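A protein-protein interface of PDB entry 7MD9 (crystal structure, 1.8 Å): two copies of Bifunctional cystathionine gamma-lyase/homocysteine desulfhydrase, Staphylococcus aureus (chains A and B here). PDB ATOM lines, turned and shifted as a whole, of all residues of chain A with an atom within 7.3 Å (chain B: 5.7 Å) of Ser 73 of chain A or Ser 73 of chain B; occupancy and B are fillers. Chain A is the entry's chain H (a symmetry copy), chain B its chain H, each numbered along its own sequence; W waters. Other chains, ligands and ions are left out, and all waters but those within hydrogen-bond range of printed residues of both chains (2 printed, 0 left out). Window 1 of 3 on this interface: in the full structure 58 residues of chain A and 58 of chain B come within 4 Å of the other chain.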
ATOM      1  N   ARG A  47      21.691  -0.690   2.862  1.00  0.00           N
ATOM      2  CA  ARG A  47      20.647  -0.083   3.689  1.00  0.00           C
ATOM      3  C   ARG A  47      19.611   0.602   2.814  1.00  0.00           C
ATOM      4  O   ARG A  47      18.401   0.432   3.008  1.00  0.00           O
ATOM      5  CB  ARG A  47      21.245   0.910   4.682  1.00  0.00           C
ATOM      6  CG  ARG A  47      20.190   1.860   5.272  1.00  0.00           C
ATOM      7  CD  ARG A  47      20.524   2.340   6.666  1.00  0.00           C
ATOM      8  NE  ARG A  47      21.857   2.920   6.788  1.00  0.00           N
ATOM      9  CZ  ARG A  47      22.250   4.055   6.218  1.00  0.00           C
ATOM     10  NH1 ARG A  47      21.409   4.774   5.474  1.00  0.00           N
ATOM     11  NH2 ARG A  47      23.495   4.478   6.406  1.00  0.00           N
ATOM     12  N   ALA A  71      10.410  -3.754   3.140  1.00  0.00           N
ATOM     13  CA  ALA A  71      10.666  -4.880   4.025  1.00  0.00           C
ATOM     14  C   ALA A  71      11.445  -4.392   5.233  1.00  0.00           C
ATOM     15  O   ALA A  71      12.492  -3.752   5.089  1.00  0.00           O
ATOM     16  CB  ALA A  71      11.434  -6.005   3.299  1.00  0.00           C
ATOM     17  N   PHE A  72      10.931  -4.698   6.421  1.00  0.00           N
ATOM     18  CA  PHE A  72      11.498  -4.246   7.675  1.00  0.00           C
ATOM     19  C   PHE A  72      11.930  -5.428   8.533  1.00  0.00           C
ATOM     20  O   PHE A  72      11.480  -6.563   8.349  1.00  0.00           O
ATOM     21  CB  PHE A  72      10.485  -3.391   8.449  1.00  0.00           C
ATOM     22  CG  PHE A  72      10.140  -2.097   7.760  1.00  0.00           C
ATOM     23  CD1 PHE A  72       9.101  -2.036   6.841  1.00  0.00           C
ATOM     24  CD2 PHE A  72      10.872  -0.953   8.012  1.00  0.00           C
ATOM     25  CE1 PHE A  72       8.789  -0.836   6.205  1.00  0.00           C
ATOM     26  CE2 PHE A  72      10.567   0.250   7.384  1.00  0.00           C
ATOM     27  CZ  PHE A  72       9.523   0.301   6.479  1.00  0.00           C
ATOM     28  N   SER A  73      12.772  -5.124   9.521  1.00  0.00           N
ATOM     29  CA  SER A  73      13.369  -6.128  10.391  1.00  0.00           C
ATOM     30  C   SER A  73      12.361  -6.823  11.306  1.00  0.00           C
ATOM     31  O   SER A  73      12.728  -7.795  11.977  1.00  0.00           O
ATOM     32  CB  SER A  73      14.456  -5.467  11.233  1.00  0.00           C
ATOM     33  OG  SER A  73      13.957  -4.266  11.801  1.00  0.00           O
ATOM     34  N   SER A  74      11.115  -6.359  11.346  1.00  0.00           N
ATOM     35  CA  SER A  74      10.079  -6.948  12.187  1.00  0.00           C
ATOM     36  C   SER A  74       8.763  -6.270  11.849  1.00  0.00           C
ATOM     37  O   SER A  74       8.736  -5.178  11.268  1.00  0.00           O
ATOM     38  CB  SER A  74      10.391  -6.774  13.678  1.00  0.00           C
ATOM     39  OG  SER A  74      10.408  -5.399  14.020  1.00  0.00           O
ATOM     40  N   GLY A  75       7.669  -6.925  12.233  1.00  0.00           N
ATOM     41  CA  GLY A  75       6.371  -6.283  12.137  1.00  0.00           C
ATOM     42  C   GLY A  75       6.318  -4.954  12.873  1.00  0.00           C
ATOM     43  O   GLY A  75       5.789  -3.968  12.351  1.00  0.00           O
ATOM     44  N   VAL A  76       6.870  -4.894  14.088  1.00  0.00           N
ATOM     45  CA  VAL A  76       6.749  -3.618  14.797  1.00  0.00           C
ATOM     46  C   VAL A  76       7.666  -2.561  14.197  1.00  0.00           C
ATOM     47  O   VAL A  76       7.395  -1.366  14.352  1.00  0.00           O
ATOM     48  CB  VAL A  76       7.005  -3.732  16.316  1.00  0.00           C
ATOM     49  CG1 VAL A  76       5.971  -4.648  16.994  1.00  0.00           C
ATOM     50  CG2 VAL A  76       8.392  -4.193  16.581  1.00  0.00           C
ATOM     51  N   ALA A  77       8.730  -2.956  13.487  1.00  0.00           N
ATOM     52  CA  ALA A  77       9.527  -1.954  12.777  1.00  0.00           C
ATOM     53  C   ALA A  77       8.749  -1.374  11.606  1.00  0.00           C
ATOM     54  O   ALA A  77       8.838  -0.175  11.331  1.00  0.00           O
ATOM     55  CB  ALA A  77      10.860  -2.557  12.305  1.00  0.00           C
ATOM     56  N   ALA A  78       7.966  -2.206  10.913  1.00  0.00           N
ATOM     57  CA  ALA A  78       7.093  -1.698   9.860  1.00  0.00           C
ATOM     58  C   ALA A  78       6.066  -0.724  10.422  1.00  0.00           C
ATOM     59  O   ALA A  78       5.802   0.334   9.831  1.00  0.00           O
ATOM     60  CB  ALA A  78       6.391  -2.857   9.157  1.00  0.00           C
ATOM     61  N   THR A 195       6.414 -12.230  10.043  1.00  0.00           N
ATOM     62  CA  THR A 195       6.810 -13.229  11.020  1.00  0.00           C
ATOM     63  C   THR A 195       5.787 -14.356  11.120  1.00  0.00           C
ATOM     64  O   THR A 195       6.124 -15.473  11.496  1.00  0.00           O
ATOM     65  CB  THR A 195       6.978 -12.556  12.409  1.00  0.00           C
ATOM     66  OG1 THR A 195       7.832 -11.413  12.272  1.00  0.00           O
ATOM     67  CG2 THR A 195       7.581 -13.516  13.427  1.00  0.00           C
ATOM     68  N1  LLP A 196       0.698  -7.090  14.172  1.00  0.00           N
ATOM     69  C2  LLP A 196       0.122  -8.264  14.276  1.00  0.00           C
ATOM     70  C2' LLP A 196      -1.318  -8.371  13.875  1.00  0.00           C
ATOM     71  C3  LLP A 196       0.818  -9.382  14.744  1.00  0.00           C
ATOM     72  O3  LLP A 196       0.157 -10.610  14.831  1.00  0.00           O
ATOM     73  C4  LLP A 196       2.157  -9.264  15.113  1.00  0.00           C
ATOM     74  C4' LLP A 196       2.895 -10.468  15.580  1.00  0.00           C
ATOM     75  C5  LLP A 196       2.748  -7.982  14.995  1.00  0.00           C
ATOM     76  C6  LLP A 196       1.959  -6.949  14.518  1.00  0.00           C
ATOM     77  C5' LLP A 196       4.190  -7.635  15.363  1.00  0.00           C
ATOM     78  OP4 LLP A 196       5.049  -8.189  14.421  1.00  0.00           O
ATOM     79  P   LLP A 196       6.558  -8.619  14.841  1.00  0.00           P
ATOM     80  OP1 LLP A 196       6.442  -9.614  15.983  1.00  0.00           O
ATOM     81  OP2 LLP A 196       7.180  -9.269  13.624  1.00  0.00           O
ATOM     82  OP3 LLP A 196       7.293  -7.374  15.284  1.00  0.00           O
ATOM     83  N   LLP A 196       4.540 -14.046  10.779  1.00  0.00           N
ATOM     84  CA  LLP A 196       3.447 -14.987  10.954  1.00  0.00           C
ATOM     85  CB  LLP A 196       2.189 -14.253  11.442  1.00  0.00           C
ATOM     86  CG  LLP A 196       2.525 -13.140  12.450  1.00  0.00           C
ATOM     87  CD  LLP A 196       3.117 -13.670  13.756  1.00  0.00           C
ATOM     88  CE  LLP A 196       3.643 -12.542  14.671  1.00  0.00           C
ATOM     89  NZ  LLP A 196       2.605 -11.683  15.217  1.00  0.00           N
ATOM     90  C   LLP A 196       3.200 -15.749   9.642  1.00  0.00           C
ATOM     91  O   LLP A 196       4.111 -16.484   9.203  1.00  0.00           O
ATOM     92  N   VAL A 204      11.500 -16.591  10.492  1.00  0.00           N
ATOM     93  CA  VAL A 204      11.887 -15.236  10.114  1.00  0.00           C
ATOM     94  C   VAL A 204      11.076 -14.255  10.952  1.00  0.00           C
ATOM     95  O   VAL A 204       9.860 -14.414  11.107  1.00  0.00           O
ATOM     96  CB  VAL A 204      11.649 -14.959   8.615  1.00  0.00           C
ATOM     97  CG1 VAL A 204      11.901 -13.475   8.295  1.00  0.00           C
ATOM     98  CG2 VAL A 204      12.527 -15.854   7.748  1.00  0.00           C
ATOM     99  N   VAL A 205      11.738 -13.238  11.485  1.00  0.00           N
ATOM    100  CA  VAL A 205      11.059 -12.079  12.053  1.00  0.00           C
ATOM    101  C   VAL A 205      11.171 -10.953  11.030  1.00  0.00           C
ATOM    102  O   VAL A 205      12.280 -10.598  10.613  1.00  0.00           O
ATOM    103  CB  VAL A 205      11.669 -11.672  13.404  1.00  0.00           C
ATOM    104  CG1 VAL A 205      11.042 -10.368  13.915  1.00  0.00           C
ATOM    105  CG2 VAL A 205      11.496 -12.797  14.422  1.00  0.00           C
ATOM    106  N   ALA A 206      10.034 -10.417  10.593  1.00  0.00           N
ATOM    107  CA  ALA A 206      10.039  -9.465   9.487  1.00  0.00           C
ATOM    108  C   ALA A 206       8.720  -8.715   9.416  1.00  0.00           C
ATOM    109  O   ALA A 206       7.675  -9.229   9.823  1.00  0.00           O
ATOM    110  CB  ALA A 206      10.293 -10.183   8.149  1.00  0.00           C
ATOM    111  N   GLY A 207       8.778  -7.506   8.865  1.00  0.00           N
ATOM    112  CA  GLY A 207       7.584  -6.739   8.535  1.00  0.00           C
ATOM    113  C   GLY A 207       7.589  -6.357   7.080  1.00  0.00           C
ATOM    114  O   GLY A 207       8.646  -6.165   6.464  1.00  0.00           O
ATOM    115  N   LEU A 208       6.393  -6.263   6.488  1.00  0.00           N
ATOM    116  CA  LEU A 208       6.229  -5.893   5.091  1.00  0.00           C
ATOM    117  C   LEU A 208       5.161  -4.816   4.984  1.00  0.00           C
ATOM    118  O   LEU A 208       4.157  -4.866   5.697  1.00  0.00           O
ATOM    119  CB  LEU A 208       5.827  -7.077   4.225  1.00  0.00           C
ATOM    120  CG  LEU A 208       6.874  -8.173   4.002  1.00  0.00           C
ATOM    121  CD1 LEU A 208       6.253  -9.315   3.238  1.00  0.00           C
ATOM    122  CD2 LEU A 208       8.066  -7.607   3.238  1.00  0.00           C
ATOM    123  N   THR A 227      16.075   5.648   9.473  1.00  0.00           N
ATOM    124  CA  THR A 227      16.028   4.962  10.759  1.00  0.00           C
ATOM    125  C   THR A 227      16.427   3.488  10.660  1.00  0.00           C
ATOM    126  O   THR A 227      16.630   2.847  11.693  1.00  0.00           O
ATOM    127  CB  THR A 227      14.631   5.095  11.384  1.00  0.00           C
ATOM    128  OG1 THR A 227      13.639   4.594  10.485  1.00  0.00           O
ATOM    129  CG2 THR A 227      14.320   6.587  11.674  1.00  0.00           C
ATOM    130  N   GLY A 228      16.528   2.940   9.457  1.00  0.00           N
ATOM    131  CA  GLY A 228      17.352   1.765   9.219  1.00  0.00           C
ATOM    132  C   GLY A 228      16.843   0.435   9.726  1.00  0.00           C
ATOM    133  O   GLY A 228      17.645  -0.490   9.884  1.00  0.00           O
ATOM    134  N   GLY A 229      15.542   0.299   9.969  1.00  0.00           N
ATOM    135  CA  GLY A 229      14.979  -0.976  10.385  1.00  0.00           C
ATOM    136  C   GLY A 229      14.730  -1.918   9.219  1.00  0.00           C
ATOM    137  O   GLY A 229      13.612  -2.399   9.035  1.00  0.00           O
ATOM    138  N   ILE A 230      15.775  -2.205   8.421  1.00  0.00           N
ATOM    139  CA  ILE A 230      15.615  -2.930   7.167  1.00  0.00           C
ATOM    140  C   ILE A 230      15.741  -4.425   7.412  1.00  0.00           C
ATOM    141  O   ILE A 230      16.482  -4.880   8.287  1.00  0.00           O
ATOM    142  CB  ILE A 230      16.658  -2.460   6.132  1.00  0.00           C
ATOM    143  CG1 ILE A 230      18.065  -2.618   6.723  1.00  0.00           C
ATOM    144  CG2 ILE A 230      16.402  -1.008   5.756  1.00  0.00           C
ATOM    145  CD1 ILE A 230      19.133  -2.932   5.713  1.00  0.00           C
ATOM    146  N   LEU A 231      15.031  -5.196   6.605  1.00  0.00           N
ATOM    147  CA  LEU A 231      15.183  -6.647   6.609  1.00  0.00           C
ATOM    148  C   LEU A 231      16.466  -7.051   5.891  1.00  0.00           C
ATOM    149  O   LEU A 231      16.779  -6.530   4.817  1.00  0.00           O
ATOM    150  CB  LEU A 231      13.977  -7.298   5.932  1.00  0.00           C
ATOM    151  CG  LEU A 231      13.899  -8.823   6.123  1.00  0.00           C
ATOM    152  CD1 LEU A 231      13.763  -9.148   7.614  1.00  0.00           C
ATOM    153  CD2 LEU A 231      12.745  -9.406   5.325  1.00  0.00           C
ATOM    154  N   GLY A 232      17.202  -7.998   6.478  1.00  0.00           N
ATOM    155  CA  GLY A 232      18.407  -8.519   5.866  1.00  0.00           C
ATOM    156  C   GLY A 232      18.133  -9.438   4.690  1.00  0.00           C
ATOM    157  O   GLY A 232      17.007  -9.886   4.473  1.00  0.00           O
ATOM    158  N   ASP A 235      16.935 -13.233   5.508  1.00  0.00           N
ATOM    159  CA  ASP A 235      15.538 -13.258   5.922  1.00  0.00           C
ATOM    160  C   ASP A 235      14.613 -12.894   4.769  1.00  0.00           C
ATOM    161  O   ASP A 235      13.522 -13.458   4.646  1.00  0.00           O
ATOM    162  CB  ASP A 235      15.331 -12.310   7.098  1.00  0.00           C
ATOM    163  CG  ASP A 235      16.050 -12.789   8.337  1.00  0.00           C
ATOM    164  OD1 ASP A 235      15.751 -13.916   8.777  1.00  0.00           O
ATOM    165  OD2 ASP A 235      16.917 -12.062   8.856  1.00  0.00           O
ATOM    166  N   ALA B  71      22.076  -5.453  19.305  1.00  0.00           N
ATOM    167  CA  ALA B  71      22.376  -5.581  17.887  1.00  0.00           C
ATOM    168  C   ALA B  71      21.175  -5.116  17.084  1.00  0.00           C
ATOM    169  O   ALA B  71      20.054  -5.590  17.299  1.00  0.00           O
ATOM    170  CB  ALA B  71      22.751  -7.032  17.517  1.00  0.00           C
ATOM    171  N   PHE B  72      21.414  -4.190  16.160  1.00  0.00           N
ATOM    172  CA  PHE B  72      20.374  -3.577  15.359  1.00  0.00           C
ATOM    173  C   PHE B  72      20.591  -3.859  13.878  1.00  0.00           C
ATOM    174  O   PHE B  72      21.694  -4.196  13.437  1.00  0.00           O
ATOM    175  CB  PHE B  72      20.335  -2.060  15.594  1.00  0.00           C
ATOM    176  CG  PHE B  72      19.937  -1.679  16.995  1.00  0.00           C
ATOM    177  CD1 PHE B  72      20.892  -1.549  17.995  1.00  0.00           C
ATOM    178  CD2 PHE B  72      18.608  -1.477  17.315  1.00  0.00           C
ATOM    179  CE1 PHE B  72      20.516  -1.199  19.290  1.00  0.00           C
ATOM    180  CE2 PHE B  72      18.224  -1.126  18.604  1.00  0.00           C
ATOM    181  CZ  PHE B  72      19.185  -0.989  19.588  1.00  0.00           C
ATOM    182  N   SER B  73      19.523  -3.654  13.107  1.00  0.00           N
ATOM    183  CA  SER B  73      19.506  -3.955  11.682  1.00  0.00           C
ATOM    184  C   SER B  73      20.423  -3.055  10.854  1.00  0.00           C
ATOM    185  O   SER B  73      20.603  -3.317   9.659  1.00  0.00           O
ATOM    186  CB  SER B  73      18.073  -3.837  11.171  1.00  0.00           C
ATOM    187  OG  SER B  73      17.500  -2.622  11.631  1.00  0.00           O
ATOM    188  N   SER B  74      21.003  -2.018  11.452  1.00  0.00           N
ATOM    189  CA  SER B  74      21.892  -1.099  10.752  1.00  0.00           C
ATOM    190  C   SER B  74      22.488  -0.153  11.780  1.00  0.00           C
ATOM    191  O   SER B  74      21.963  -0.001  12.890  1.00  0.00           O
ATOM    192  CB  SER B  74      21.149  -0.300   9.674  1.00  0.00           C
ATOM    193  OG  SER B  74      20.157   0.521  10.266  1.00  0.00           O
ATOM    194  N   GLY B  75      23.587   0.492  11.392  1.00  0.00           N
ATOM    195  CA  GLY B  75      24.127   1.559  12.215  1.00  0.00           C
ATOM    196  C   GLY B  75      23.108   2.648  12.507  1.00  0.00           C
ATOM    197  O   GLY B  75      22.993   3.112  13.645  1.00  0.00           O
ATOM    198  N   ALA B  77      19.929   2.376  12.627  1.00  0.00           N
ATOM    199  CA  ALA B  77      18.909   1.879  13.551  1.00  0.00           C
ATOM    200  C   ALA B  77      19.412   1.918  14.985  1.00  0.00           C
ATOM    201  O   ALA B  77      18.651   2.233  15.904  1.00  0.00           O
ATOM    202  CB  ALA B  77      18.475   0.456  13.162  1.00  0.00           C
ATOM    203  N   VAL B 205      24.950  -5.443   6.932  1.00  0.00           N
ATOM    204  CA  VAL B 205      24.533  -4.130   7.415  1.00  0.00           C
ATOM    205  C   VAL B 205      24.008  -4.325   8.833  1.00  0.00           C
ATOM    206  O   VAL B 205      23.101  -5.137   9.056  1.00  0.00           O
ATOM    207  CB  VAL B 205      23.465  -3.506   6.502  1.00  0.00           C
ATOM    208  CG1 VAL B 205      22.934  -2.197   7.102  1.00  0.00           C
ATOM    209  CG2 VAL B 205      24.034  -3.274   5.105  1.00  0.00           C
ATOM    210  N   ALA B 206      24.595  -3.621   9.798  1.00  0.00           N
ATOM    211  CA  ALA B 206      24.281  -3.877  11.200  1.00  0.00           C
ATOM    212  C   ALA B 206      24.760  -2.733  12.076  1.00  0.00           C
ATOM    213  O   ALA B 206      25.726  -2.040  11.746  1.00  0.00           O
ATOM    214  CB  ALA B 206      24.928  -5.191  11.674  1.00  0.00           C
ATOM    215  N   GLY B 207      24.090  -2.564  13.214  1.00  0.00           N
ATOM    216  CA  GLY B 207      24.540  -1.652  14.258  1.00  0.00           C
ATOM    217  C   GLY B 207      24.690  -2.381  15.565  1.00  0.00           C
ATOM    218  O   GLY B 207      23.979  -3.355  15.848  1.00  0.00           O
ATOM    219  N   THR B 227      10.241  -0.943  18.888  1.00  0.00           N
ATOM    220  CA  THR B 227      10.365  -0.429  17.529  1.00  0.00           C
ATOM    221  C   THR B 227      11.055  -1.413  16.583  1.00  0.00           C
ATOM    222  O   THR B 227      11.041  -1.196  15.370  1.00  0.00           O
ATOM    223  CB  THR B 227      11.105   0.917  17.532  1.00  0.00           C
ATOM    224  OG1 THR B 227      12.383   0.774  18.158  1.00  0.00           O
ATOM    225  CG2 THR B 227      10.287   1.970  18.326  1.00  0.00           C
ATOM    226  N   GLY B 228      11.665  -2.468  17.104  1.00  0.00           N
ATOM    227  CA  GLY B 228      11.898  -3.677  16.329  1.00  0.00           C
ATOM    228  C   GLY B 228      12.980  -3.637  15.273  1.00  0.00           C
ATOM    229  O   GLY B 228      12.959  -4.474  14.365  1.00  0.00           O
ATOM    230  N   GLY B 229      13.930  -2.711  15.366  1.00  0.00           N
ATOM    231  CA  GLY B 229      15.040  -2.667  14.427  1.00  0.00           C
ATOM    232  C   GLY B 229      16.143  -3.653  14.773  1.00  0.00           C
ATOM    233  O   GLY B 229      17.302  -3.264  14.918  1.00  0.00           O
ATOM    234  N   ILE B 230      15.800  -4.947  14.898  1.00  0.00           N
ATOM    235  CA  ILE B 230      16.724  -5.947  15.419  1.00  0.00           C
ATOM    236  C   ILE B 230      17.530  -6.553  14.281  1.00  0.00           C
ATOM    237  O   ILE B 230      17.054  -6.695  13.151  1.00  0.00           O
ATOM    238  CB  ILE B 230      15.960  -7.045  16.187  1.00  0.00           C
ATOM    239  CG1 ILE B 230      14.895  -7.657  15.268  1.00  0.00           C
ATOM    240  CG2 ILE B 230      15.311  -6.456  17.430  1.00  0.00           C
ATOM    241  CD1 ILE B 230      14.611  -9.110  15.527  1.00  0.00           C
ATOM    242  N   LEU B 231      18.755  -6.942  14.594  1.00  0.00           N
ATOM    243  CA  LEU B 231      19.579  -7.693  13.654  1.00  0.00           C
ATOM    244  C   LEU B 231      19.120  -9.145  13.583  1.00  0.00           C
ATOM    245  O   LEU B 231      18.854  -9.774  14.610  1.00  0.00           O
ATOM    246  CB  LEU B 231      21.046  -7.628  14.081  1.00  0.00           C
ATOM    247  CG  LEU B 231      22.031  -8.149  13.020  1.00  0.00           C
ATOM    248  CD1 LEU B 231      21.929  -7.288  11.757  1.00  0.00           C
ATOM    249  CD2 LEU B 231      23.450  -8.163  13.565  1.00  0.00           C
HETATM  250  O   HOH W   1      19.002  -5.865   8.757  1.00  0.00           O
HETATM  251  O   HOH W   2      15.759  -8.473  11.507  1.00  0.00           O
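O of Gly 228 of chain A is in hydrogen-bond range of OG of Ser 73 of chain B, 2.8 Å away.
O of Gly 228 of chain A sits at hydrogen-bond distance from OG of Ser 74 of chain B (2.7 Å).
The backbone NH (N) of Ala 77 of chain B sits close to the backbone carbonyl oxygen (O) of Thr 227 of chain A, 3.5 Å away.
The backbone carbonyl oxygen (O) of Thr 227 of chain B sits close to the backbone NH (N) of Ala 77 of chain A.
The backbone carbonyl oxygen of Gly 228 of chain B lies within hydrogen-bond range of the side-chain hydroxyl of Ser 73 of chain A (2.8 Å).
The backbone carbonyl oxygen of Gly 228 of chain B is in hydrogen-bond range of the side-chain hydroxyl of Ser 74 of chain A, at 2.7 Å.
The backbone carbonyl oxygen of Gly 229 of chain B is in hydrogen-bond range of the backbone NH of Ser 73 of chain B, 2.9 Å away.
OG of Ser 74 of chain B sits at hydrogen-bond distance from N of Ala 77 of chain B.
N of Ser 73 of chain A lies within hydrogen-bond range of O of Gly 229 of chain A.
OG of Ser 74 of chain A sits at hydrogen-bond distance from N of Ala 77 of chain A.
The backbone NH of Gly 207 of chain A sits close to the backbone carbonyl oxygen of Ser 74 of chain A.
OP3 of LLP 196 of chain A sits at hydrogen-bond distance from the backbone NH (N) of Val 76 of chain A (2.8 Å).
Among the printed residues, merely in contact across the chains: Gly 229 of chain A with Ser 73 of chain B (3.3 Å), Ser 73 of chain A with Gly 229 of chain B (3.3 Å), Ser 73 of chain A with Ile 230 of chain B (3.5 Å), Ile 230 of chain A with Ser 73 of chain B (3.5 Å), Ala 77 of chain A with Gly 228 of chain B (3.5 Å), Gly 228 of chain A with Ala 77 of chain B (3.5 Å), Val 76 of chain A with Gly 228 of chain B (3.6 Å), Val 76 of chain A with Thr 227 of chain B (3.8 Å) and Ser 73 of chain A with Ser 73 of chain B (3.9 Å).
Of chain B, only Ser 73, Gly 228, Gly 229 and Ile 230 come within 4 Å of Ser 73 of chain A.
Of the printed residues of chain B, Val 76 of chain A touches Thr 227 (3.8 Å) and Gly 228 (3.6 Å).
Of the printed residues of chain B, Thr 227 of chain A touches Ala 77 (3.1 Å).
Of the printed residues of chain B, Gly 228 of chain A touches Ser 73, Ser 74 and Ala 77.
Of chain A, only Ser 73, Gly 228, Gly 229 and Ile 230 come within 4 Å of Ser 73 of chain B.
Printed residues of chain A within 4 Å of Gly 228 of chain B: Ser 73 (2.8 Å), Ser 74 (2.7 Å), Val 76 (3.6 Å) and Ala 77 (3.5 Å).
Printed residues of chain A within 4 Å of Gly 229 of chain B: Ser 73 (3.3 Å).
The nearest residue of chain B that does not touch Ser 73 of chain A is Thr 227 of chain B (5.5 Å).
The nearest residue of chain A that does not touch Ser 73 of chain B is Thr 227 of chain A (5.5 Å).
The nearest printed residue of chain B that does not touch Ser 74 of chain A is Thr 227 of chain B (4.5 Å).
Printed residues of chain A that touch a printed residue of chain B: Ser 73, Ser 74, Val 76, Ala 77, Thr 227, Gly 228, Gly 229 and Ile 230.
Hydrophobic or aromatic side chains of chain A that line the printed part of chain B: Val 76, Ala 77 and Ile 230.
Ser 73 of chain B touches its own counterpart, Ser 73 of chain A.
Ser 73 of chain A touches Gly 228 of chain B, and with the chains exchanged Gly 228 of chain A touches Ser 73 of chain B.
Ser 74 of chain A touches Gly 228 of chain B, and with the chains exchanged Gly 228 of chain A touches Ser 74 of chain B.
Ala 77 of chain A touches Thr 227 of chain B, and with the chains exchanged Thr 227 of chain A touches Ala 77 of chain B.
14 positions are printed for both chains.
Water W1 bridges the backbone carbonyl oxygen (O) of Ile 230 of chain A and the backbone carbonyl oxygen (O) of Ser 73 of chain B.
Water W2 lies within hydrogen-bond range of the backbone carbonyl oxygen of Ile 230 of chain B (2.7 Å) and the backbone carbonyl oxygen of Ser 73 of chain A (3.1 Å).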
